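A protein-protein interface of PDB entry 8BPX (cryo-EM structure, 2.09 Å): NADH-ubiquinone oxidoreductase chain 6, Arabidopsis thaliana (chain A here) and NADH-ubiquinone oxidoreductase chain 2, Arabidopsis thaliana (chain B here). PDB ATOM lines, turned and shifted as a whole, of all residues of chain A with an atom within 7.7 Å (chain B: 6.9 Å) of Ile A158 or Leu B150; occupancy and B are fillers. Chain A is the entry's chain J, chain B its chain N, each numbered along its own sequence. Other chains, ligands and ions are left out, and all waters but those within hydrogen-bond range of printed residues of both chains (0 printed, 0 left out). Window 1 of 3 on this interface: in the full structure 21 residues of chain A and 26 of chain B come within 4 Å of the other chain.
Leu B150 touches two residues of chain A.
Of the printed residues of chain B, Val A161 touches Leu B154 (3.6 Å).
Printed residues of chain A within 4 Å of Leu B154: Ile A158 and Val A161.
Met B139 touches none of the printed residues of chain A.
The nearest residue of chain B that does not touch Ile A158 is Glu B153 (4.4 Å).
The nearest residue of chain A that does not touch Leu B150 is Val A154 (4.2 Å).
The nearest printed residue of chain A that does not touch Asp B144 is Tyr A148 (6.2 Å).
N of Ile B146 sits at hydrogen-bond distance from OD2 of Asp B144, at 2.6 Å.
Of the 16 printed residues of chain B, 6 touch a printed residue of chain A.
Hydrophobic or aromatic side chains of chain B that line the printed part of chain A: Ile B146, Ala B147, Leu B150, Leu B154 and Leu B157.
Along chain B the printed residues that touch a printed residue of chain A span positions 144 to 157.
Among the printed residues, no Asp or Glu carboxylate lies within 4 Å of a Lys or Arg side-chain nitrogen of the other chain.
Among the printed residues, merely in contact across the chains: Trp A151 with Asp B144 (3.96 Å), Trp A151 with Ile B146 (3.5 Å), Trp A151 with Ala B147 (3.4 Å), Trp A151 with Leu B150 (3.6 Å), Ile A158 with Leu B150 (3.7 Å), Ile A158 with Leu B154 (3.8 Å), Ile A158 with Leu B157 (3.6 Å) and Val A161 with Leu B154 (3.6 Å).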
ATOM      1  N   TYR A 148     -30.809   2.580  30.501  1.00  0.00           N
ATOM      2  CA  TYR A 148     -29.826   1.729  29.846  1.00  0.00           C
ATOM      3  C   TYR A 148     -30.034   1.727  28.337  1.00  0.00           C
ATOM      4  O   TYR A 148     -29.833   0.715  27.663  1.00  0.00           O
ATOM      5  CB  TYR A 148     -29.876   0.319  30.432  1.00  0.00           C
ATOM      6  CG  TYR A 148     -29.544   0.318  31.905  1.00  0.00           C
ATOM      7  CD1 TYR A 148     -28.225   0.320  32.332  1.00  0.00           C
ATOM      8  CD2 TYR A 148     -30.545   0.354  32.868  1.00  0.00           C
ATOM      9  CE1 TYR A 148     -27.908   0.341  33.673  1.00  0.00           C
ATOM     10  CE2 TYR A 148     -30.236   0.370  34.218  1.00  0.00           C
ATOM     11  CZ  TYR A 148     -28.913   0.365  34.611  1.00  0.00           C
ATOM     12  OH  TYR A 148     -28.587   0.380  35.946  1.00  0.00           O
ATOM     13  N   VAL A 150     -28.378   3.069  25.877  1.00  0.00           N
ATOM     14  CA  VAL A 150     -27.205   2.907  25.018  1.00  0.00           C
ATOM     15  C   VAL A 150     -26.991   1.439  24.659  1.00  0.00           C
ATOM     16  O   VAL A 150     -26.677   1.107  23.509  1.00  0.00           O
ATOM     17  CB  VAL A 150     -25.959   3.516  25.688  1.00  0.00           C
ATOM     18  CG1 VAL A 150     -24.728   3.293  24.823  1.00  0.00           C
ATOM     19  CG2 VAL A 150     -26.169   4.998  25.943  1.00  0.00           C
ATOM     20  N   TRP A 151     -27.141   0.540  25.637  1.00  0.00           N
ATOM     21  CA  TRP A 151     -26.972  -0.888  25.374  1.00  0.00           C
ATOM     22  C   TRP A 151     -28.040  -1.402  24.409  1.00  0.00           C
ATOM     23  O   TRP A 151     -27.755  -2.216  23.521  1.00  0.00           O
ATOM     24  CB  TRP A 151     -27.003  -1.660  26.695  1.00  0.00           C
ATOM     25  CG  TRP A 151     -25.978  -1.192  27.698  1.00  0.00           C
ATOM     26  CD1 TRP A 151     -24.886  -0.412  27.452  1.00  0.00           C
ATOM     27  CD2 TRP A 151     -25.935  -1.509  29.095  1.00  0.00           C
ATOM     28  NE1 TRP A 151     -24.176  -0.209  28.609  1.00  0.00           N
ATOM     29  CE2 TRP A 151     -24.799  -0.873  29.632  1.00  0.00           C
ATOM     30  CE3 TRP A 151     -26.752  -2.260  29.944  1.00  0.00           C
ATOM     31  CZ2 TRP A 151     -24.457  -0.967  30.980  1.00  0.00           C
ATOM     32  CZ3 TRP A 151     -26.410  -2.354  31.283  1.00  0.00           C
ATOM     33  CH2 TRP A 151     -25.272  -1.711  31.786  1.00  0.00           C
ATOM     34  N   PHE A 152     -29.274  -0.933  24.583  1.00  0.00           N
ATOM     35  CA  PHE A 152     -30.370  -1.185  23.651  1.00  0.00           C
ATOM     36  C   PHE A 152     -29.978  -0.811  22.215  1.00  0.00           C
ATOM     37  O   PHE A 152     -30.119  -1.612  21.276  1.00  0.00           O
ATOM     38  CB  PHE A 152     -31.574  -0.380  24.161  1.00  0.00           C
ATOM     39  CG  PHE A 152     -32.788  -0.403  23.288  1.00  0.00           C
ATOM     40  CD1 PHE A 152     -33.359  -1.592  22.878  1.00  0.00           C
ATOM     41  CD2 PHE A 152     -33.404   0.789  22.933  1.00  0.00           C
ATOM     42  CE1 PHE A 152     -34.496  -1.590  22.099  1.00  0.00           C
ATOM     43  CE2 PHE A 152     -34.541   0.794  22.152  1.00  0.00           C
ATOM     44  CZ  PHE A 152     -35.087  -0.395  21.737  1.00  0.00           C
ATOM     45  N   LEU A 153     -29.444   0.397  22.036  1.00  0.00           N
ATOM     46  CA  LEU A 153     -29.073   0.845  20.695  1.00  0.00           C
ATOM     47  C   LEU A 153     -27.889   0.052  20.132  1.00  0.00           C
ATOM     48  O   LEU A 153     -27.842  -0.239  18.928  1.00  0.00           O
ATOM     49  CB  LEU A 153     -28.772   2.341  20.719  1.00  0.00           C
ATOM     50  CG  LEU A 153     -29.973   3.234  21.035  1.00  0.00           C
ATOM     51  CD1 LEU A 153     -29.597   4.701  20.930  1.00  0.00           C
ATOM     52  CD2 LEU A 153     -31.157   2.909  20.121  1.00  0.00           C
ATOM     53  N   VAL A 154     -26.924  -0.309  20.978  1.00  0.00           N
ATOM     54  CA  VAL A 154     -25.812  -1.133  20.499  1.00  0.00           C
ATOM     55  C   VAL A 154     -26.323  -2.491  20.019  1.00  0.00           C
ATOM     56  O   VAL A 154     -25.840  -3.037  19.019  1.00  0.00           O
ATOM     57  CB  VAL A 154     -24.733  -1.280  21.589  1.00  0.00           C
ATOM     58  CG1 VAL A 154     -23.667  -2.276  21.152  1.00  0.00           C
ATOM     59  CG2 VAL A 154     -24.095   0.070  21.883  1.00  0.00           C
ATOM     60  N   SER A 155     -27.315  -3.048  20.719  1.00  0.00           N
ATOM     61  CA  SER A 155     -27.933  -4.286  20.249  1.00  0.00           C
ATOM     62  C   SER A 155     -28.574  -4.091  18.877  1.00  0.00           C
ATOM     63  O   SER A 155     -28.512  -4.984  18.015  1.00  0.00           O
ATOM     64  CB  SER A 155     -28.966  -4.777  21.262  1.00  0.00           C
ATOM     65  OG  SER A 155     -30.226  -4.174  21.035  1.00  0.00           O
ATOM     66  N   SER A 156     -29.211  -2.935  18.663  1.00  0.00           N
ATOM     67  CA  SER A 156     -29.722  -2.628  17.326  1.00  0.00           C
ATOM     68  C   SER A 156     -28.605  -2.654  16.285  1.00  0.00           C
ATOM     69  O   SER A 156     -28.791  -3.161  15.170  1.00  0.00           O
ATOM     70  CB  SER A 156     -30.418  -1.269  17.311  1.00  0.00           C
ATOM     71  OG  SER A 156     -29.490  -0.209  17.205  1.00  0.00           O
ATOM     72  N   LEU A 157     -27.443  -2.097  16.627  1.00  0.00           N
ATOM     73  CA  LEU A 157     -26.312  -2.135  15.699  1.00  0.00           C
ATOM     74  C   LEU A 157     -25.902  -3.572  15.389  1.00  0.00           C
ATOM     75  O   LEU A 157     -25.560  -3.903  14.244  1.00  0.00           O
ATOM     76  CB  LEU A 157     -25.130  -1.352  16.269  1.00  0.00           C
ATOM     77  CG  LEU A 157     -25.217   0.174  16.221  1.00  0.00           C
ATOM     78  CD1 LEU A 157     -23.915   0.793  16.709  1.00  0.00           C
ATOM     79  CD2 LEU A 157     -25.552   0.650  14.812  1.00  0.00           C
ATOM     80  N   ILE A 158     -25.931  -4.434  16.405  1.00  0.00           N
ATOM     81  CA  ILE A 158     -25.602  -5.845  16.209  1.00  0.00           C
ATOM     82  C   ILE A 158     -26.569  -6.487  15.211  1.00  0.00           C
ATOM     83  O   ILE A 158     -26.159  -7.224  14.299  1.00  0.00           O
ATOM     84  CB  ILE A 158     -25.601  -6.571  17.570  1.00  0.00           C
ATOM     85  CG1 ILE A 158     -24.319  -6.258  18.347  1.00  0.00           C
ATOM     86  CG2 ILE A 158     -25.779  -8.063  17.401  1.00  0.00           C
ATOM     87  CD1 ILE A 158     -24.401  -6.591  19.823  1.00  0.00           C
ATOM     88  N   LEU A 159     -27.862  -6.193  15.352  1.00  0.00           N
ATOM     89  CA  LEU A 159     -28.842  -6.744  14.416  1.00  0.00           C
ATOM     90  C   LEU A 159     -28.623  -6.216  12.999  1.00  0.00           C
ATOM     91  O   LEU A 159     -28.768  -6.960  12.020  1.00  0.00           O
ATOM     92  CB  LEU A 159     -30.261  -6.444  14.894  1.00  0.00           C
ATOM     93  CG  LEU A 159     -30.664  -7.154  16.190  1.00  0.00           C
ATOM     94  CD1 LEU A 159     -32.061  -6.743  16.612  1.00  0.00           C
ATOM     95  CD2 LEU A 159     -30.554  -8.671  16.049  1.00  0.00           C
ATOM     96  N   LEU A 160     -28.273  -4.932  12.872  1.00  0.00           N
ATOM     97  CA  LEU A 160     -27.973  -4.375  11.554  1.00  0.00           C
ATOM     98  C   LEU A 160     -26.802  -5.106  10.904  1.00  0.00           C
ATOM     99  O   LEU A 160     -26.830  -5.399   9.698  1.00  0.00           O
ATOM    100  CB  LEU A 160     -27.675  -2.879  11.670  1.00  0.00           C
ATOM    101  CG  LEU A 160     -27.198  -2.173  10.396  1.00  0.00           C
ATOM    102  CD1 LEU A 160     -28.271  -2.219   9.337  1.00  0.00           C
ATOM    103  CD2 LEU A 160     -26.800  -0.733  10.684  1.00  0.00           C
ATOM    104  N   VAL A 161     -25.764  -5.401  11.691  1.00  0.00           N
ATOM    105  CA  VAL A 161     -24.642  -6.181  11.175  1.00  0.00           C
ATOM    106  C   VAL A 161     -25.126  -7.537  10.682  1.00  0.00           C
ATOM    107  O   VAL A 161     -24.699  -8.014   9.625  1.00  0.00           O
ATOM    108  CB  VAL A 161     -23.543  -6.332  12.245  1.00  0.00           C
ATOM    109  CG1 VAL A 161     -22.501  -7.347  11.794  1.00  0.00           C
ATOM    110  CG2 VAL A 161     -22.891  -4.994  12.525  1.00  0.00           C
ATOM    111  N   ALA A 162     -26.013  -8.184  11.443  1.00  0.00           N
ATOM    112  CA  ALA A 162     -26.532  -9.482  11.013  1.00  0.00           C
ATOM    113  C   ALA A 162     -27.223  -9.381   9.656  1.00  0.00           C
ATOM    114  O   ALA A 162     -26.997 -10.210   8.769  1.00  0.00           O
ATOM    115  CB  ALA A 162     -27.492 -10.048  12.061  1.00  0.00           C
ATOM    116  N   MET A 163     -28.065  -8.359   9.478  1.00  0.00           N
ATOM    117  CA  MET A 163     -28.776  -8.191   8.210  1.00  0.00           C
ATOM    118  C   MET A 163     -27.802  -7.993   7.050  1.00  0.00           C
ATOM    119  O   MET A 163     -27.895  -8.667   6.008  1.00  0.00           O
ATOM    120  CB  MET A 163     -29.744  -7.007   8.309  1.00  0.00           C
ATOM    121  CG  MET A 163     -30.555  -7.000   9.591  1.00  0.00           C
ATOM    122  SD  MET A 163     -31.513  -5.511   9.933  1.00  0.00           S
ATOM    123  CE  MET A 163     -32.623  -5.461   8.544  1.00  0.00           C
ATOM    124  N   ILE A 164     -26.844  -7.079   7.226  1.00  0.00           N
ATOM    125  CA  ILE A 164     -25.884  -6.793   6.164  1.00  0.00           C
ATOM    126  C   ILE A 164     -25.087  -8.042   5.816  1.00  0.00           C
ATOM    127  O   ILE A 164     -24.905  -8.374   4.638  1.00  0.00           O
ATOM    128  CB  ILE A 164     -24.958  -5.632   6.569  1.00  0.00           C
ATOM    129  CG1 ILE A 164     -25.717  -4.305   6.560  1.00  0.00           C
ATOM    130  CG2 ILE A 164     -23.747  -5.572   5.646  1.00  0.00           C
ATOM    131  CD1 ILE A 164     -24.919  -3.149   7.122  1.00  0.00           C
ATOM    132  N   GLY B 135     -17.799  -0.364  17.373  1.00  0.00           N
ATOM    133  CA  GLY B 135     -17.787  -1.348  18.441  1.00  0.00           C
ATOM    134  C   GLY B 135     -16.541  -1.269  19.303  1.00  0.00           C
ATOM    135  O   GLY B 135     -16.618  -1.364  20.526  1.00  0.00           O
ATOM    136  N   MET B 139     -15.942  -0.447  23.133  1.00  0.00           N
ATOM    137  CA  MET B 139     -15.168  -1.365  23.964  1.00  0.00           C
ATOM    138  C   MET B 139     -14.223  -0.602  24.881  1.00  0.00           C
ATOM    139  O   MET B 139     -14.113  -0.913  26.072  1.00  0.00           O
ATOM    140  CB  MET B 139     -14.365  -2.344  23.103  1.00  0.00           C
ATOM    141  CG  MET B 139     -15.154  -3.447  22.424  1.00  0.00           C
ATOM    142  SD  MET B 139     -14.141  -4.459  21.330  1.00  0.00           S
ATOM    143  CE  MET B 139     -12.932  -5.087  22.492  1.00  0.00           C
ATOM    144  N   ASP B 144     -18.627  -1.677  32.438  1.00  0.00           N
ATOM    145  CA  ASP B 144     -19.558  -2.643  33.000  1.00  0.00           C
ATOM    146  C   ASP B 144     -19.459  -3.902  32.154  1.00  0.00           C
ATOM    147  O   ASP B 144     -19.193  -3.832  30.951  1.00  0.00           O
ATOM    148  CB  ASP B 144     -20.991  -2.084  33.024  1.00  0.00           C
ATOM    149  CG  ASP B 144     -22.010  -3.069  33.582  1.00  0.00           C
ATOM    150  OD1 ASP B 144     -22.612  -2.761  34.631  1.00  0.00           O
ATOM    151  OD2 ASP B 144     -22.236  -4.133  32.968  1.00  0.00           O
ATOM    152  N   LEU B 145     -19.668  -5.056  32.793  1.00  0.00           N
ATOM    153  CA  LEU B 145     -19.518  -6.324  32.086  1.00  0.00           C
ATOM    154  C   LEU B 145     -20.492  -6.426  30.918  1.00  0.00           C
ATOM    155  O   LEU B 145     -20.149  -6.960  29.857  1.00  0.00           O
ATOM    156  CB  LEU B 145     -19.715  -7.491  33.050  1.00  0.00           C
ATOM    157  CG  LEU B 145     -18.774  -7.557  34.254  1.00  0.00           C
ATOM    158  CD1 LEU B 145     -19.454  -8.260  35.416  1.00  0.00           C
ATOM    159  CD2 LEU B 145     -17.462  -8.226  33.892  1.00  0.00           C
ATOM    160  N   ILE B 146     -21.707  -5.902  31.093  1.00  0.00           N
ATOM    161  CA  ILE B 146     -22.721  -5.965  30.044  1.00  0.00           C
ATOM    162  C   ILE B 146     -22.287  -5.157  28.825  1.00  0.00           C
ATOM    163  O   ILE B 146     -22.325  -5.642  27.686  1.00  0.00           O
ATOM    164  CB  ILE B 146     -24.071  -5.469  30.591  1.00  0.00           C
ATOM    165  CG1 ILE B 146     -24.549  -6.380  31.726  1.00  0.00           C
ATOM    166  CG2 ILE B 146     -25.097  -5.357  29.471  1.00  0.00           C
ATOM    167  CD1 ILE B 146     -25.698  -5.809  32.533  1.00  0.00           C
ATOM    168  N   ALA B 147     -21.883  -3.905  29.052  1.00  0.00           N
ATOM    169  CA  ALA B 147     -21.437  -3.050  27.955  1.00  0.00           C
ATOM    170  C   ALA B 147     -20.221  -3.645  27.263  1.00  0.00           C
ATOM    171  O   ALA B 147     -20.126  -3.637  26.026  1.00  0.00           O
ATOM    172  CB  ALA B 147     -21.125  -1.648  28.482  1.00  0.00           C
ATOM    173  N   MET B 148     -19.282  -4.169  28.052  1.00  0.00           N
ATOM    174  CA  MET B 148     -18.090  -4.791  27.494  1.00  0.00           C
ATOM    175  C   MET B 148     -18.458  -5.955  26.585  1.00  0.00           C
ATOM    176  O   MET B 148     -17.961  -6.058  25.458  1.00  0.00           O
ATOM    177  CB  MET B 148     -17.171  -5.249  28.625  1.00  0.00           C
ATOM    178  CG  MET B 148     -15.879  -5.902  28.169  1.00  0.00           C
ATOM    179  SD  MET B 148     -14.931  -6.539  29.564  1.00  0.00           S
ATOM    180  CE  MET B 148     -15.878  -7.993  29.991  1.00  0.00           C
ATOM    181  N   TYR B 149     -19.358  -6.827  27.052  1.00  0.00           N
ATOM    182  CA  TYR B 149     -19.768  -7.968  26.242  1.00  0.00           C
ATOM    183  C   TYR B 149     -20.445  -7.521  24.954  1.00  0.00           C
ATOM    184  O   TYR B 149     -20.162  -8.060  23.879  1.00  0.00           O
ATOM    185  CB  TYR B 149     -20.700  -8.880  27.037  1.00  0.00           C
ATOM    186  CG  TYR B 149     -21.284  -9.995  26.199  1.00  0.00           C
ATOM    187  CD1 TYR B 149     -20.517 -11.099  25.847  1.00  0.00           C
ATOM    188  CD2 TYR B 149     -22.594  -9.940  25.755  1.00  0.00           C
ATOM    189  CE1 TYR B 149     -21.044 -12.118  25.082  1.00  0.00           C
ATOM    190  CE2 TYR B 149     -23.129 -10.957  24.986  1.00  0.00           C
ATOM    191  CZ  TYR B 149     -22.348 -12.042  24.654  1.00  0.00           C
ATOM    192  OH  TYR B 149     -22.871 -13.056  23.893  1.00  0.00           O
ATOM    193  N   LEU B 150     -21.347  -6.541  25.042  1.00  0.00           N
ATOM    194  CA  LEU B 150     -22.071  -6.109  23.849  1.00  0.00           C
ATOM    195  C   LEU B 150     -21.117  -5.537  22.805  1.00  0.00           C
ATOM    196  O   LEU B 150     -21.206  -5.866  21.613  1.00  0.00           O
ATOM    197  CB  LEU B 150     -23.139  -5.084  24.228  1.00  0.00           C
ATOM    198  CG  LEU B 150     -24.355  -5.618  24.989  1.00  0.00           C
ATOM    199  CD1 LEU B 150     -25.371  -4.518  25.186  1.00  0.00           C
ATOM    200  CD2 LEU B 150     -24.980  -6.810  24.271  1.00  0.00           C
ATOM    201  N   ALA B 151     -20.191  -4.679  23.239  1.00  0.00           N
ATOM    202  CA  ALA B 151     -19.246  -4.079  22.303  1.00  0.00           C
ATOM    203  C   ALA B 151     -18.325  -5.135  21.693  1.00  0.00           C
ATOM    204  O   ALA B 151     -18.058  -5.119  20.479  1.00  0.00           O
ATOM    205  CB  ALA B 151     -18.452  -2.986  23.014  1.00  0.00           C
ATOM    206  N   ILE B 152     -17.857  -6.080  22.516  1.00  0.00           N
ATOM    207  CA  ILE B 152     -17.036  -7.176  22.014  1.00  0.00           C
ATOM    208  C   ILE B 152     -17.791  -7.970  20.956  1.00  0.00           C
ATOM    209  O   ILE B 152     -17.232  -8.331  19.917  1.00  0.00           O
ATOM    210  CB  ILE B 152     -16.577  -8.077  23.177  1.00  0.00           C
ATOM    211  CG1 ILE B 152     -15.541  -7.357  24.044  1.00  0.00           C
ATOM    212  CG2 ILE B 152     -16.012  -9.388  22.660  1.00  0.00           C
ATOM    213  CD1 ILE B 152     -15.047  -8.188  25.202  1.00  0.00           C
ATOM    214  N   GLU B 153     -19.074  -8.245  21.199  1.00  0.00           N
ATOM    215  CA  GLU B 153     -19.858  -9.029  20.248  1.00  0.00           C
ATOM    216  C   GLU B 153     -20.063  -8.282  18.934  1.00  0.00           C
ATOM    217  O   GLU B 153     -20.005  -8.890  17.860  1.00  0.00           O
ATOM    218  CB  GLU B 153     -21.205  -9.408  20.856  1.00  0.00           C
ATOM    219  CG  GLU B 153     -21.123 -10.429  21.974  1.00  0.00           C
ATOM    220  CD  GLU B 153     -20.183 -11.578  21.663  1.00  0.00           C
ATOM    221  OE1 GLU B 153     -20.585 -12.495  20.922  1.00  0.00           O
ATOM    222  OE2 GLU B 153     -19.040 -11.566  22.168  1.00  0.00           O
ATOM    223  N   LEU B 154     -20.339  -6.978  18.998  1.00  0.00           N
ATOM    224  CA  LEU B 154     -20.480  -6.198  17.768  1.00  0.00           C
ATOM    225  C   LEU B 154     -19.208  -6.281  16.928  1.00  0.00           C
ATOM    226  O   LEU B 154     -19.245  -6.599  15.723  1.00  0.00           O
ATOM    227  CB  LEU B 154     -20.812  -4.746  18.112  1.00  0.00           C
ATOM    228  CG  LEU B 154     -20.777  -3.688  17.004  1.00  0.00           C
ATOM    229  CD1 LEU B 154     -21.629  -4.097  15.814  1.00  0.00           C
ATOM    230  CD2 LEU B 154     -21.217  -2.335  17.536  1.00  0.00           C
ATOM    231  N   GLN B 155     -18.067  -6.027  17.572  1.00  0.00           N
ATOM    232  CA  GLN B 155     -16.771  -6.153  16.916  1.00  0.00           C
ATOM    233  C   GLN B 155     -16.577  -7.543  16.304  1.00  0.00           C
ATOM    234  O   GLN B 155     -16.180  -7.679  15.136  1.00  0.00           O
ATOM    235  CB  GLN B 155     -15.687  -5.830  17.947  1.00  0.00           C
ATOM    236  CG  GLN B 155     -14.280  -5.771  17.440  1.00  0.00           C
ATOM    237  CD  GLN B 155     -13.426  -6.828  18.090  1.00  0.00           C
ATOM    238  OE1 GLN B 155     -13.791  -8.001  18.118  1.00  0.00           O
ATOM    239  NE2 GLN B 155     -12.279  -6.419  18.624  1.00  0.00           N
ATOM    240  N   SER B 156     -16.885  -8.585  17.078  1.00  0.00           N
ATOM    241  CA  SER B 156     -16.654  -9.953  16.629  1.00  0.00           C
ATOM    242  C   SER B 156     -17.520 -10.307  15.426  1.00  0.00           C
ATOM    243  O   SER B 156     -17.050 -10.963  14.493  1.00  0.00           O
ATOM    244  CB  SER B 156     -16.913 -10.932  17.773  1.00  0.00           C
ATOM    245  OG  SER B 156     -15.795 -11.022  18.635  1.00  0.00           O
ATOM    246  N   LEU B 157     -18.793  -9.913  15.446  1.00  0.00           N
ATOM    247  CA  LEU B 157     -19.682 -10.244  14.337  1.00  0.00           C
ATOM    248  C   LEU B 157     -19.228  -9.556  13.055  1.00  0.00           C
ATOM    249  O   LEU B 157     -19.228 -10.169  11.974  1.00  0.00           O
ATOM    250  CB  LEU B 157     -21.120  -9.869  14.691  1.00  0.00           C
ATOM    251  CG  LEU B 157     -21.698 -10.685  15.852  1.00  0.00           C
ATOM    252  CD1 LEU B 157     -23.025 -10.126  16.342  1.00  0.00           C
ATOM    253  CD2 LEU B 157     -21.825 -12.151  15.482  1.00  0.00           C
